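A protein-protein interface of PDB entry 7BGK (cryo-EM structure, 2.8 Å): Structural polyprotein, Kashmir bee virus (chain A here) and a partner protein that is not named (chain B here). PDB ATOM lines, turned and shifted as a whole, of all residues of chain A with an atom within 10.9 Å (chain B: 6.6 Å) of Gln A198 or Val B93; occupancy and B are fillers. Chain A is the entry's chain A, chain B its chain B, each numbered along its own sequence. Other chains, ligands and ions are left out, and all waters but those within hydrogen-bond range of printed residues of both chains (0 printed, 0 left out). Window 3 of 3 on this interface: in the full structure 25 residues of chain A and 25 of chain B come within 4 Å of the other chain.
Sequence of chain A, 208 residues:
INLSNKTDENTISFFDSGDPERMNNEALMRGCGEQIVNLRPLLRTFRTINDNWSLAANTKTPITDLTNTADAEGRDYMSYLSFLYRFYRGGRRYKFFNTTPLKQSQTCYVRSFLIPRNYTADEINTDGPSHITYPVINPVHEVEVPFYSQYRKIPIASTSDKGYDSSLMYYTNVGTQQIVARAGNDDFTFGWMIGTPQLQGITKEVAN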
ATOM      1  N   ASP A  71      10.227 -17.285  17.570  1.00  0.00           N
ATOM      2  CA  ASP A  71       9.537 -16.352  18.452  1.00  0.00           C
ATOM      3  C   ASP A  71      10.434 -15.863  19.576  1.00  0.00           C
ATOM      4  O   ASP A  71      10.241 -14.754  20.083  1.00  0.00           O
ATOM      5  CB  ASP A  71       8.285 -17.013  19.022  1.00  0.00           C
ATOM      6  CG  ASP A  71       7.230 -17.275  17.964  1.00  0.00           C
ATOM      7  OD1 ASP A  71       7.172 -16.517  16.975  1.00  0.00           O
ATOM      8  OD2 ASP A  71       6.454 -18.241  18.122  1.00  0.00           O
ATOM      9  N   ALA A  72      11.412 -16.667  19.983  1.00  0.00           N
ATOM     10  CA  ALA A  72      12.302 -16.275  21.063  1.00  0.00           C
ATOM     11  C   ALA A  72      13.438 -15.380  20.592  1.00  0.00           C
ATOM     12  O   ALA A  72      14.000 -14.636  21.403  1.00  0.00           O
ATOM     13  CB  ALA A  72      12.874 -17.518  21.739  1.00  0.00           C
ATOM     14  N   GLU A  73      13.779 -15.427  19.305  1.00  0.00           N
ATOM     15  CA  GLU A  73      14.945 -14.704  18.811  1.00  0.00           C
ATOM     16  C   GLU A  73      14.704 -13.201  18.803  1.00  0.00           C
ATOM     17  O   GLU A  73      15.551 -12.423  19.251  1.00  0.00           O
ATOM     18  CB  GLU A  73      15.302 -15.196  17.410  1.00  0.00           C
ATOM     19  CG  GLU A  73      15.756 -16.636  17.355  1.00  0.00           C
ATOM     20  CD  GLU A  73      16.081 -17.088  15.945  1.00  0.00           C
ATOM     21  OE1 GLU A  73      15.773 -16.341  14.994  1.00  0.00           O
ATOM     22  OE2 GLU A  73      16.645 -18.190  15.787  1.00  0.00           O
ATOM     23  N   GLY A  74      13.556 -12.774  18.289  1.00  0.00           N
ATOM     24  CA  GLY A  74      13.283 -11.364  18.130  1.00  0.00           C
ATOM     25  C   GLY A  74      13.738 -10.782  16.818  1.00  0.00           C
ATOM     26  O   GLY A  74      14.009  -9.579  16.745  1.00  0.00           O
ATOM     27  N   ARG A  75      13.821 -11.595  15.770  1.00  0.00           N
ATOM     28  CA  ARG A  75      14.361 -11.160  14.491  1.00  0.00           C
ATOM     29  C   ARG A  75      13.286 -10.578  13.584  1.00  0.00           C
ATOM     30  O   ARG A  75      13.528  -9.577  12.905  1.00  0.00           O
ATOM     31  CB  ARG A  75      15.060 -12.330  13.799  1.00  0.00           C
ATOM     32  CG  ARG A  75      15.640 -11.998  12.445  1.00  0.00           C
ATOM     33  CD  ARG A  75      16.111 -13.240  11.727  1.00  0.00           C
ATOM     34  NE  ARG A  75      16.352 -12.998  10.311  1.00  0.00           N
ATOM     35  CZ  ARG A  75      16.767 -13.925   9.456  1.00  0.00           C
ATOM     36  NH1 ARG A  75      16.991 -15.164   9.867  1.00  0.00           N
ATOM     37  NH2 ARG A  75      16.959 -13.612   8.186  1.00  0.00           N
ATOM     38  N   SER A  79       7.798 -11.463  16.234  1.00  0.00           N
ATOM     39  CA  SER A  79       8.501 -11.873  17.438  1.00  0.00           C
ATOM     40  C   SER A  79       9.022 -10.698  18.247  1.00  0.00           C
ATOM     41  O   SER A  79       8.865 -10.677  19.470  1.00  0.00           O
ATOM     42  CB  SER A  79       9.670 -12.780  17.067  1.00  0.00           C
ATOM     43  OG  SER A  79      10.326 -13.267  18.218  1.00  0.00           O
ATOM     44  N   TYR A  80       9.634  -9.716  17.589  1.00  0.00           N
ATOM     45  CA  TYR A  80      10.129  -8.545  18.297  1.00  0.00           C
ATOM     46  C   TYR A  80       8.999  -7.811  19.000  1.00  0.00           C
ATOM     47  O   TYR A  80       9.137  -7.406  20.159  1.00  0.00           O
ATOM     48  CB  TYR A  80      10.847  -7.622  17.318  1.00  0.00           C
ATOM     49  CG  TYR A  80      11.722  -6.576  17.955  1.00  0.00           C
ATOM     50  CD1 TYR A  80      12.955  -6.904  18.489  1.00  0.00           C
ATOM     51  CD2 TYR A  80      11.330  -5.253  17.991  1.00  0.00           C
ATOM     52  CE1 TYR A  80      13.754  -5.948  19.057  1.00  0.00           C
ATOM     53  CE2 TYR A  80      12.124  -4.297  18.556  1.00  0.00           C
ATOM     54  CZ  TYR A  80      13.330  -4.642  19.084  1.00  0.00           C
ATOM     55  OH  TYR A  80      14.105  -3.660  19.641  1.00  0.00           O
ATOM     56  N   PHE A  83       7.149  -9.275  22.421  1.00  0.00           N
ATOM     57  CA  PHE A  83       7.703  -9.085  23.751  1.00  0.00           C
ATOM     58  C   PHE A  83       7.138  -7.862  24.451  1.00  0.00           C
ATOM     59  O   PHE A  83       7.455  -7.635  25.623  1.00  0.00           O
ATOM     60  CB  PHE A  83       9.221  -8.979  23.661  1.00  0.00           C
ATOM     61  CG  PHE A  83       9.900 -10.281  23.399  1.00  0.00           C
ATOM     62  CD1 PHE A  83      10.261 -11.109  24.437  1.00  0.00           C
ATOM     63  CD2 PHE A  83      10.180 -10.678  22.113  1.00  0.00           C
ATOM     64  CE1 PHE A  83      10.882 -12.301  24.193  1.00  0.00           C
ATOM     65  CE2 PHE A  83      10.801 -11.870  21.868  1.00  0.00           C
ATOM     66  CZ  PHE A  83      11.153 -12.682  22.910  1.00  0.00           C
ATOM     67  N   LEU A  84       6.318  -7.077  23.763  1.00  0.00           N
ATOM     68  CA  LEU A  84       5.611  -5.959  24.360  1.00  0.00           C
ATOM     69  C   LEU A  84       4.201  -6.312  24.799  1.00  0.00           C
ATOM     70  O   LEU A  84       3.557  -5.497  25.464  1.00  0.00           O
ATOM     71  CB  LEU A  84       5.534  -4.796  23.371  1.00  0.00           C
ATOM     72  CG  LEU A  84       6.813  -4.080  22.979  1.00  0.00           C
ATOM     73  CD1 LEU A  84       6.536  -3.222  21.781  1.00  0.00           C
ATOM     74  CD2 LEU A  84       7.317  -3.246  24.118  1.00  0.00           C
ATOM     75  N   ILE A 194       2.928  -4.407  27.774  1.00  0.00           N
ATOM     76  CA  ILE A 194       3.750  -4.655  28.948  1.00  0.00           C
ATOM     77  C   ILE A 194       5.127  -4.061  28.692  1.00  0.00           C
ATOM     78  O   ILE A 194       5.348  -3.382  27.686  1.00  0.00           O
ATOM     79  CB  ILE A 194       3.850  -6.155  29.274  1.00  0.00           C
ATOM     80  CG1 ILE A 194       4.371  -6.923  28.069  1.00  0.00           C
ATOM     81  CG2 ILE A 194       2.514  -6.690  29.712  1.00  0.00           C
ATOM     82  CD1 ILE A 194       4.846  -8.257  28.391  1.00  0.00           C
ATOM     83  N   GLY A 195       6.050  -4.310  29.601  1.00  0.00           N
ATOM     84  CA  GLY A 195       7.386  -3.777  29.486  1.00  0.00           C
ATOM     85  C   GLY A 195       8.258  -4.540  28.521  1.00  0.00           C
ATOM     86  O   GLY A 195       7.940  -5.638  28.069  1.00  0.00           O
ATOM     87  N   THR A 196       9.365  -3.940  28.214  1.00  0.00           N
ATOM     88  CA  THR A 196      10.346  -4.463  27.282  1.00  0.00           C
ATOM     89  C   THR A 196      11.309  -5.424  27.967  1.00  0.00           C
ATOM     90  O   THR A 196      11.519  -5.345  29.180  1.00  0.00           O
ATOM     91  CB  THR A 196      11.140  -3.315  26.673  1.00  0.00           C
ATOM     92  OG1 THR A 196      11.764  -2.564  27.719  1.00  0.00           O
ATOM     93  CG2 THR A 196      10.246  -2.416  25.905  1.00  0.00           C
ATOM     94  N   PRO A 197      11.896  -6.351  27.208  1.00  0.00           N
ATOM     95  CA  PRO A 197      13.032  -7.121  27.721  1.00  0.00           C
ATOM     96  C   PRO A 197      14.365  -6.467  27.402  1.00  0.00           C
ATOM     97  O   PRO A 197      14.399  -5.386  26.807  1.00  0.00           O
ATOM     98  CB  PRO A 197      12.871  -8.464  27.008  1.00  0.00           C
ATOM     99  CG  PRO A 197      12.255  -8.113  25.719  1.00  0.00           C
ATOM    100  CD  PRO A 197      11.447  -6.866  25.905  1.00  0.00           C
ATOM    101  N   GLN A 198      15.469  -7.100  27.791  1.00  0.00           N
ATOM    102  CA  GLN A 198      16.769  -6.623  27.356  1.00  0.00           C
ATOM    103  C   GLN A 198      16.976  -6.957  25.883  1.00  0.00           C
ATOM    104  O   GLN A 198      16.297  -7.813  25.311  1.00  0.00           O
ATOM    105  CB  GLN A 198      17.907  -7.237  28.176  1.00  0.00           C
ATOM    106  CG  GLN A 198      18.056  -6.756  29.613  1.00  0.00           C
ATOM    107  CD  GLN A 198      17.027  -7.328  30.531  1.00  0.00           C
ATOM    108  OE1 GLN A 198      16.233  -6.606  31.128  1.00  0.00           O
ATOM    109  NE2 GLN A 198      17.053  -8.642  30.678  1.00  0.00           N
ATOM    110  N   LEU A 199      17.920  -6.260  25.263  1.00  0.00           N
ATOM    111  CA  LEU A 199      18.313  -6.521  23.889  1.00  0.00           C
ATOM    112  C   LEU A 199      19.745  -7.033  23.849  1.00  0.00           C
ATOM    113  O   LEU A 199      20.578  -6.669  24.681  1.00  0.00           O
ATOM    114  CB  LEU A 199      18.186  -5.272  23.020  1.00  0.00           C
ATOM    115  CG  LEU A 199      16.769  -4.792  22.720  1.00  0.00           C
ATOM    116  CD1 LEU A 199      16.811  -3.459  22.027  1.00  0.00           C
ATOM    117  CD2 LEU A 199      16.010  -5.785  21.878  1.00  0.00           C
ATOM    118  N   GLN A 200      20.021  -7.884  22.868  1.00  0.00           N
ATOM    119  CA  GLN A 200      21.325  -8.502  22.683  1.00  0.00           C
ATOM    120  C   GLN A 200      22.018  -7.838  21.504  1.00  0.00           C
ATOM    121  O   GLN A 200      21.473  -7.808  20.396  1.00  0.00           O
ATOM    122  CB  GLN A 200      21.184 -10.004  22.446  1.00  0.00           C
ATOM    123  CG  GLN A 200      22.449 -10.796  22.638  1.00  0.00           C
ATOM    124  CD  GLN A 200      22.207 -12.283  22.591  1.00  0.00           C
ATOM    125  OE1 GLN A 200      21.318 -12.803  23.262  1.00  0.00           O
ATOM    126  NE2 GLN A 200      22.995 -12.978  21.787  1.00  0.00           N
ATOM    127  N   GLY A 201      23.210  -7.304  21.744  1.00  0.00           N
ATOM    128  CA  GLY A 201      23.939  -6.617  20.703  1.00  0.00           C
ATOM    129  C   GLY A 201      25.115  -7.396  20.157  1.00  0.00           C
ATOM    130  O   GLY A 201      25.037  -8.611  19.962  1.00  0.00           O
ATOM    131  N   SER B  90      17.178  -3.600  39.791  1.00  0.00           N
ATOM    132  CA  SER B  90      18.480  -3.613  39.145  1.00  0.00           C
ATOM    133  C   SER B  90      18.403  -3.175  37.689  1.00  0.00           C
ATOM    134  O   SER B  90      17.482  -3.548  36.959  1.00  0.00           O
ATOM    135  CB  SER B  90      19.093  -5.006  39.248  1.00  0.00           C
ATOM    136  OG  SER B  90      20.341  -5.079  38.594  1.00  0.00           O
ATOM    137  N   ARG B  91      19.386  -2.369  37.281  1.00  0.00           N
ATOM    138  CA  ARG B  91      19.423  -1.850  35.917  1.00  0.00           C
ATOM    139  C   ARG B  91      19.381  -2.972  34.892  1.00  0.00           C
ATOM    140  O   ARG B  91      18.583  -2.935  33.951  1.00  0.00           O
ATOM    141  CB  ARG B  91      20.669  -0.983  35.729  1.00  0.00           C
ATOM    142  CG  ARG B  91      20.794  -0.319  34.375  1.00  0.00           C
ATOM    143  CD  ARG B  91      19.725   0.702  34.165  1.00  0.00           C
ATOM    144  NE  ARG B  91      19.856   1.423  32.902  1.00  0.00           N
ATOM    145  CZ  ARG B  91      20.528   2.558  32.746  1.00  0.00           C
ATOM    146  NH1 ARG B  91      21.158   3.115  33.763  1.00  0.00           N
ATOM    147  NH2 ARG B  91      20.572   3.137  31.560  1.00  0.00           N
ATOM    148  N   TYR B  92      20.217  -3.989  35.063  1.00  0.00           N
ATOM    149  CA  TYR B  92      20.270  -5.103  34.134  1.00  0.00           C
ATOM    150  C   TYR B  92      20.045  -6.415  34.868  1.00  0.00           C
ATOM    151  O   TYR B  92      20.187  -6.510  36.088  1.00  0.00           O
ATOM    152  CB  TYR B  92      21.613  -5.162  33.398  1.00  0.00           C
ATOM    153  CG  TYR B  92      22.045  -3.865  32.770  1.00  0.00           C
ATOM    154  CD1 TYR B  92      21.637  -3.520  31.494  1.00  0.00           C
ATOM    155  CD2 TYR B  92      22.864  -2.986  33.450  1.00  0.00           C
ATOM    156  CE1 TYR B  92      22.031  -2.342  30.922  1.00  0.00           C
ATOM    157  CE2 TYR B  92      23.263  -1.803  32.883  1.00  0.00           C
ATOM    158  CZ  TYR B  92      22.842  -1.486  31.617  1.00  0.00           C
ATOM    159  OH  TYR B  92      23.239  -0.302  31.046  1.00  0.00           O
ATOM    160  N   VAL B  93      19.688  -7.431  34.090  1.00  0.00           N
ATOM    161  CA  VAL B  93      19.604  -8.809  34.551  1.00  0.00           C
ATOM    162  C   VAL B  93      20.276  -9.650  33.478  1.00  0.00           C
ATOM    163  O   VAL B  93      19.697  -9.885  32.412  1.00  0.00           O
ATOM    164  CB  VAL B  93      18.165  -9.267  34.796  1.00  0.00           C
ATOM    165  CG1 VAL B  93      18.118 -10.739  35.088  1.00  0.00           C
ATOM    166  CG2 VAL B  93      17.555  -8.492  35.919  1.00  0.00           C
ATOM    167  N   LEU B  94      21.497 -10.094  33.746  1.00  0.00           N
ATOM    168  CA  LEU B  94      22.254 -10.855  32.768  1.00  0.00           C
ATOM    169  C   LEU B  94      22.045 -12.350  32.902  1.00  0.00           C
ATOM    170  O   LEU B  94      22.235 -13.076  31.921  1.00  0.00           O
ATOM    171  CB  LEU B  94      23.744 -10.542  32.902  1.00  0.00           C
ATOM    172  CG  LEU B  94      24.125  -9.066  32.904  1.00  0.00           C
ATOM    173  CD1 LEU B  94      25.588  -8.899  33.185  1.00  0.00           C
ATOM    174  CD2 LEU B  94      23.781  -8.428  31.587  1.00  0.00           C
ATOM    175  N   ASP B  95      21.651 -12.824  34.079  1.00  0.00           N
ATOM    176  CA  ASP B  95      21.483 -14.245  34.321  1.00  0.00           C
ATOM    177  C   ASP B  95      20.272 -14.450  35.218  1.00  0.00           C
ATOM    178  O   ASP B  95      19.820 -13.531  35.903  1.00  0.00           O
ATOM    179  CB  ASP B  95      22.733 -14.847  34.966  1.00  0.00           C
ATOM    180  CG  ASP B  95      23.987 -14.686  34.130  1.00  0.00           C
ATOM    181  OD1 ASP B  95      23.890 -14.711  32.886  1.00  0.00           O
ATOM    182  OD2 ASP B  95      25.075 -14.517  34.719  1.00  0.00           O
ATOM    183  N   ARG B  96      19.749 -15.674  35.208  1.00  0.00           N
ATOM    184  CA  ARG B  96      18.595 -16.013  36.030  1.00  0.00           C
ATOM    185  C   ARG B  96      18.960 -16.302  37.477  1.00  0.00           C
ATOM    186  O   ARG B  96      18.080 -16.243  38.342  1.00  0.00           O
ATOM    187  CB  ARG B  96      17.861 -17.216  35.445  1.00  0.00           C
ATOM    188  CG  ARG B  96      17.284 -16.977  34.071  1.00  0.00           C
ATOM    189  CD  ARG B  96      16.562 -18.195  33.555  1.00  0.00           C
ATOM    190  NE  ARG B  96      16.803 -18.401  32.134  1.00  0.00           N
ATOM    191  CZ  ARG B  96      16.674 -19.570  31.518  1.00  0.00           C
ATOM    192  NH1 ARG B  96      16.303 -20.645  32.194  1.00  0.00           N
ATOM    193  NH2 ARG B  96      16.920 -19.664  30.221  1.00  0.00           N
ATOM    194  N   ASN B  98      20.436 -14.287  39.123  1.00  0.00           N
ATOM    195  CA  ASN B  98      20.613 -12.922  39.592  1.00  0.00           C
ATOM    196  C   ASN B  98      19.410 -12.093  39.163  1.00  0.00           C
ATOM    197  O   ASN B  98      19.578 -11.053  38.515  1.00  0.00           O
ATOM    198  CB  ASN B  98      21.897 -12.305  39.041  1.00  0.00           C
ATOM    199  CG  ASN B  98      22.272 -11.022  39.753  1.00  0.00           C
ATOM    200  OD1 ASN B  98      21.468 -10.458  40.495  1.00  0.00           O
ATOM    201  ND2 ASN B  98      23.479 -10.530  39.500  1.00  0.00           N
ATOM    202  N   PRO B  99      18.194 -12.508  39.491  1.00  0.00           N
ATOM    203  CA  PRO B  99      17.011 -11.848  38.945  1.00  0.00           C
ATOM    204  C   PRO B  99      16.642 -10.611  39.755  1.00  0.00           C
ATOM    205  O   PRO B  99      17.312 -10.236  40.713  1.00  0.00           O
ATOM    206  CB  PRO B  99      15.945 -12.931  39.053  1.00  0.00           C
ATOM    207  CG  PRO B  99      16.327 -13.706  40.246  1.00  0.00           C
ATOM    208  CD  PRO B  99      17.822 -13.594  40.412  1.00  0.00           C
ATOM    209  N   GLN B 100      15.550  -9.976  39.345  1.00  0.00           N
ATOM    210  CA  GLN B 100      15.067  -8.804  40.053  1.00  0.00           C
ATOM    211  C   GLN B 100      14.443  -9.209  41.379  1.00  0.00           C
ATOM    212  O   GLN B 100      13.725 -10.207  41.470  1.00  0.00           O
ATOM    213  CB  GLN B 100      14.050  -8.048  39.206  1.00  0.00           C
ATOM    214  CG  GLN B 100      14.622  -7.389  37.981  1.00  0.00           C
ATOM    215  CD  GLN B 100      15.527  -6.236  38.302  1.00  0.00           C
ATOM    216  OE1 GLN B 100      15.838  -5.976  39.462  1.00  0.00           O
ATOM    217  NE2 GLN B 100      15.960  -5.533  37.274  1.00  0.00           N
ATOM    218  N   GLU B 162      12.453 -15.209  29.291  1.00  0.00           N
ATOM    219  CA  GLU B 162      12.822 -13.928  28.704  1.00  0.00           C
ATOM    220  C   GLU B 162      11.662 -12.946  28.684  1.00  0.00           C
ATOM    221  O   GLU B 162      11.892 -11.735  28.595  1.00  0.00           O
ATOM    222  CB  GLU B 162      13.352 -14.138  27.289  1.00  0.00           C
ATOM    223  CG  GLU B 162      12.431 -14.929  26.378  1.00  0.00           C
ATOM    224  CD  GLU B 162      12.780 -16.400  26.305  1.00  0.00           C
ATOM    225  OE1 GLU B 162      13.500 -16.894  27.197  1.00  0.00           O
ATOM    226  OE2 GLU B 162      12.328 -17.064  25.352  1.00  0.00           O
ATOM    227  N   ILE B 165       8.546 -10.433  33.912  1.00  0.00           N
ATOM    228  CA  ILE B 165       8.920  -9.202  34.599  1.00  0.00           C
ATOM    229  C   ILE B 165      10.131  -9.449  35.482  1.00  0.00           C
ATOM    230  O   ILE B 165      11.006  -8.588  35.627  1.00  0.00           O
ATOM    231  CB  ILE B 165       7.720  -8.657  35.393  1.00  0.00           C
ATOM    232  CG1 ILE B 165       8.000  -7.238  35.871  1.00  0.00           C
ATOM    233  CG2 ILE B 165       7.400  -9.549  36.549  1.00  0.00           C
ATOM    234  CD1 ILE B 165       6.808  -6.535  36.404  1.00  0.00           C
ATOM    235  N   ILE B 166      10.180 -10.616  36.117  1.00  0.00           N
ATOM    236  CA  ILE B 166      11.442 -11.147  36.599  1.00  0.00           C
ATOM    237  C   ILE B 166      12.269 -11.533  35.385  1.00  0.00           C
ATOM    238  O   ILE B 166      11.732 -11.986  34.366  1.00  0.00           O
ATOM    239  CB  ILE B 166      11.193 -12.346  37.531  1.00  0.00           C
ATOM    240  CG1 ILE B 166      10.208 -11.982  38.638  1.00  0.00           C
ATOM    241  CG2 ILE B 166      12.469 -12.832  38.146  1.00  0.00           C
ATOM    242  CD1 ILE B 166      10.598 -10.790  39.458  1.00  0.00           C
ATOM    243  N   TYR B 167      13.578 -11.342  35.472  1.00  0.00           N
ATOM    244  CA  TYR B 167      14.509 -11.605  34.381  1.00  0.00           C
ATOM    245  C   TYR B 167      14.473 -10.534  33.299  1.00  0.00           C
ATOM    246  O   TYR B 167      14.836 -10.809  32.153  1.00  0.00           O
ATOM    247  CB  TYR B 167      14.266 -12.969  33.728  1.00  0.00           C
ATOM    248  CG  TYR B 167      14.154 -14.118  34.696  1.00  0.00           C
ATOM    249  CD1 TYR B 167      15.072 -14.281  35.714  1.00  0.00           C
ATOM    250  CD2 TYR B 167      13.141 -15.049  34.578  1.00  0.00           C
ATOM    251  CE1 TYR B 167      14.977 -15.330  36.593  1.00  0.00           C
ATOM    252  CE2 TYR B 167      13.038 -16.101  35.452  1.00  0.00           C
ATOM    253  CZ  TYR B 167      13.959 -16.237  36.458  1.00  0.00           C
ATOM    254  OH  TYR B 167      13.863 -17.289  37.337  1.00  0.00           O
ATOM    255  N   THR B 168      14.044  -9.320  33.624  1.00  0.00           N
ATOM    256  CA  THR B 168      14.171  -8.177  32.732  1.00  0.00           C
ATOM    257  C   THR B 168      14.736  -7.000  33.512  1.00  0.00           C
ATOM    258  O   THR B 168      15.006  -7.086  34.712  1.00  0.00           O
ATOM    259  CB  THR B 168      12.845  -7.800  32.058  1.00  0.00           C
ATOM    260  OG1 THR B 168      13.116  -6.926  30.960  1.00  0.00           O
ATOM    261  CG2 THR B 168      11.913  -7.099  33.008  1.00  0.00           C
ATOM    262  N   SER B 169      14.920  -5.892  32.809  1.00  0.00           N
ATOM    263  CA  SER B 169      15.613  -4.735  33.343  1.00  0.00           C
ATOM    264  C   SER B 169      14.673  -3.834  34.133  1.00  0.00           C
ATOM    265  O   SER B 169      13.455  -4.011  34.154  1.00  0.00           O
ATOM    266  CB  SER B 169      16.256  -3.934  32.221  1.00  0.00           C
ATOM    267  OG  SER B 169      15.395  -3.806  31.107  1.00  0.00           O
ATOM    268  N   ARG B 170      15.272  -2.841  34.787  1.00  0.00           N
ATOM    269  CA  ARG B 170      14.497  -1.827  35.485  1.00  0.00           C
ATOM    270  C   ARG B 170      13.613  -1.053  34.520  1.00  0.00           C
ATOM    271  O   ARG B 170      12.450  -0.762  34.825  1.00  0.00           O
ATOM    272  CB  ARG B 170      15.443  -0.888  36.220  1.00  0.00           C
ATOM    273  CG  ARG B 170      14.769   0.105  37.105  1.00  0.00           C
ATOM    274  CD  ARG B 170      15.769   0.816  37.968  1.00  0.00           C
ATOM    275  NE  ARG B 170      16.757   1.542  37.182  1.00  0.00           N
ATOM    276  CZ  ARG B 170      17.923   1.957  37.657  1.00  0.00           C
ATOM    277  NH1 ARG B 170      18.256   1.721  38.914  1.00  0.00           N
ATOM    278  NH2 ARG B 170      18.756   2.609  36.870  1.00  0.00           N
ATOM    279  N   GLY B 172      12.488  -2.236  31.816  1.00  0.00           N
ATOM    280  CA  GLY B 172      11.484  -3.178  31.383  1.00  0.00           C
ATOM    281  C   GLY B 172      10.422  -3.379  32.437  1.00  0.00           C
ATOM    282  O   GLY B 172       9.227  -3.369  32.139  1.00  0.00           O
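Of the printed residues of chain B, Ala A72 touches Glu B162 (3.7 Å).
Of the printed residues of chain B, Phe A83 touches Glu B162.
Of the printed residues of chain B, Thr A196 touches Thr B168 (2.9 Å) and Gly B172 (3.1 Å).
Gln A198 touches just these residues of chain B: Val B93 (3.4 Å), Tyr B167 (3.4 Å), Thr B168 (2.8 Å) and Ser B169 (2.2 Å).
Val B93 touches just one residue of chain A: Gln A198.
No residue of chain A comes within 4 Å of Leu B94.
Of the printed residues of chain A, Tyr B167 touches Gln A198.
Of chain A, only Thr A196, Pro A197 and Gln A198 come within 4 Å of Thr B168.
Of chain A, only Gln A198 (2.2 Å) comes within 4 Å of Ser B169.
The nearest printed residue of chain B that does not touch Gly A195 is Thr B168 (5.9 Å).
The side-chain amide nitrogen of Gln B100 sits at hydrogen-bond distance from the backbone carbonyl oxygen of Thr B168 (3.1 Å).
The side-chain hydroxyl (OG) of Ser B169 is in hydrogen-bond range of the backbone NH (N) of Gly B172 (3.4 Å).
Hydrophobic or aromatic side chains of chain A within 4 Å of the printed part of chain B: Ala A72, Phe A83 and Pro A197.
Along chain A the printed residues that touch a printed residue of chain B span positions 72 to 198.
Among the printed residues, no Asp or Glu carboxylate lies within 4 Å of a Lys or Arg side-chain nitrogen of the other chain.
The backbone carbonyl oxygen of Thr A196 lies within hydrogen-bond range of the side-chain hydroxyl of Thr B168.
The side-chain amide nitrogen (NE2) of Gln A198 lies within hydrogen-bond range of the backbone carbonyl oxygen (O) of Val B93, 3.4 Å away.
The side-chain amide nitrogen (NE2) of Gln A198 lies within hydrogen-bond range of the backbone carbonyl oxygen (O) of Tyr B167 (3.4 Å).
OG1 of Thr B168 sits close to OE1 of Gln A198 (3.1 Å).
The side-chain amide oxygen (OE1) of Gln A198 lies close to the side-chain hydroxyl (OG) of Ser B169, 2.9 Å away.
Among the printed residues, pairs that only touch across the chains: Thr A196 with Gly B172 (3.1 Å), Pro A197 with Thr B168 (3.2 Å), Gly A195 with Gly B172 (3.3 Å), Ala A72 with Glu B162 (3.7 Å), Phe A83 with Glu B162 (3.8 Å) and Pro A197 with Glu B162 (3.8 Å).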
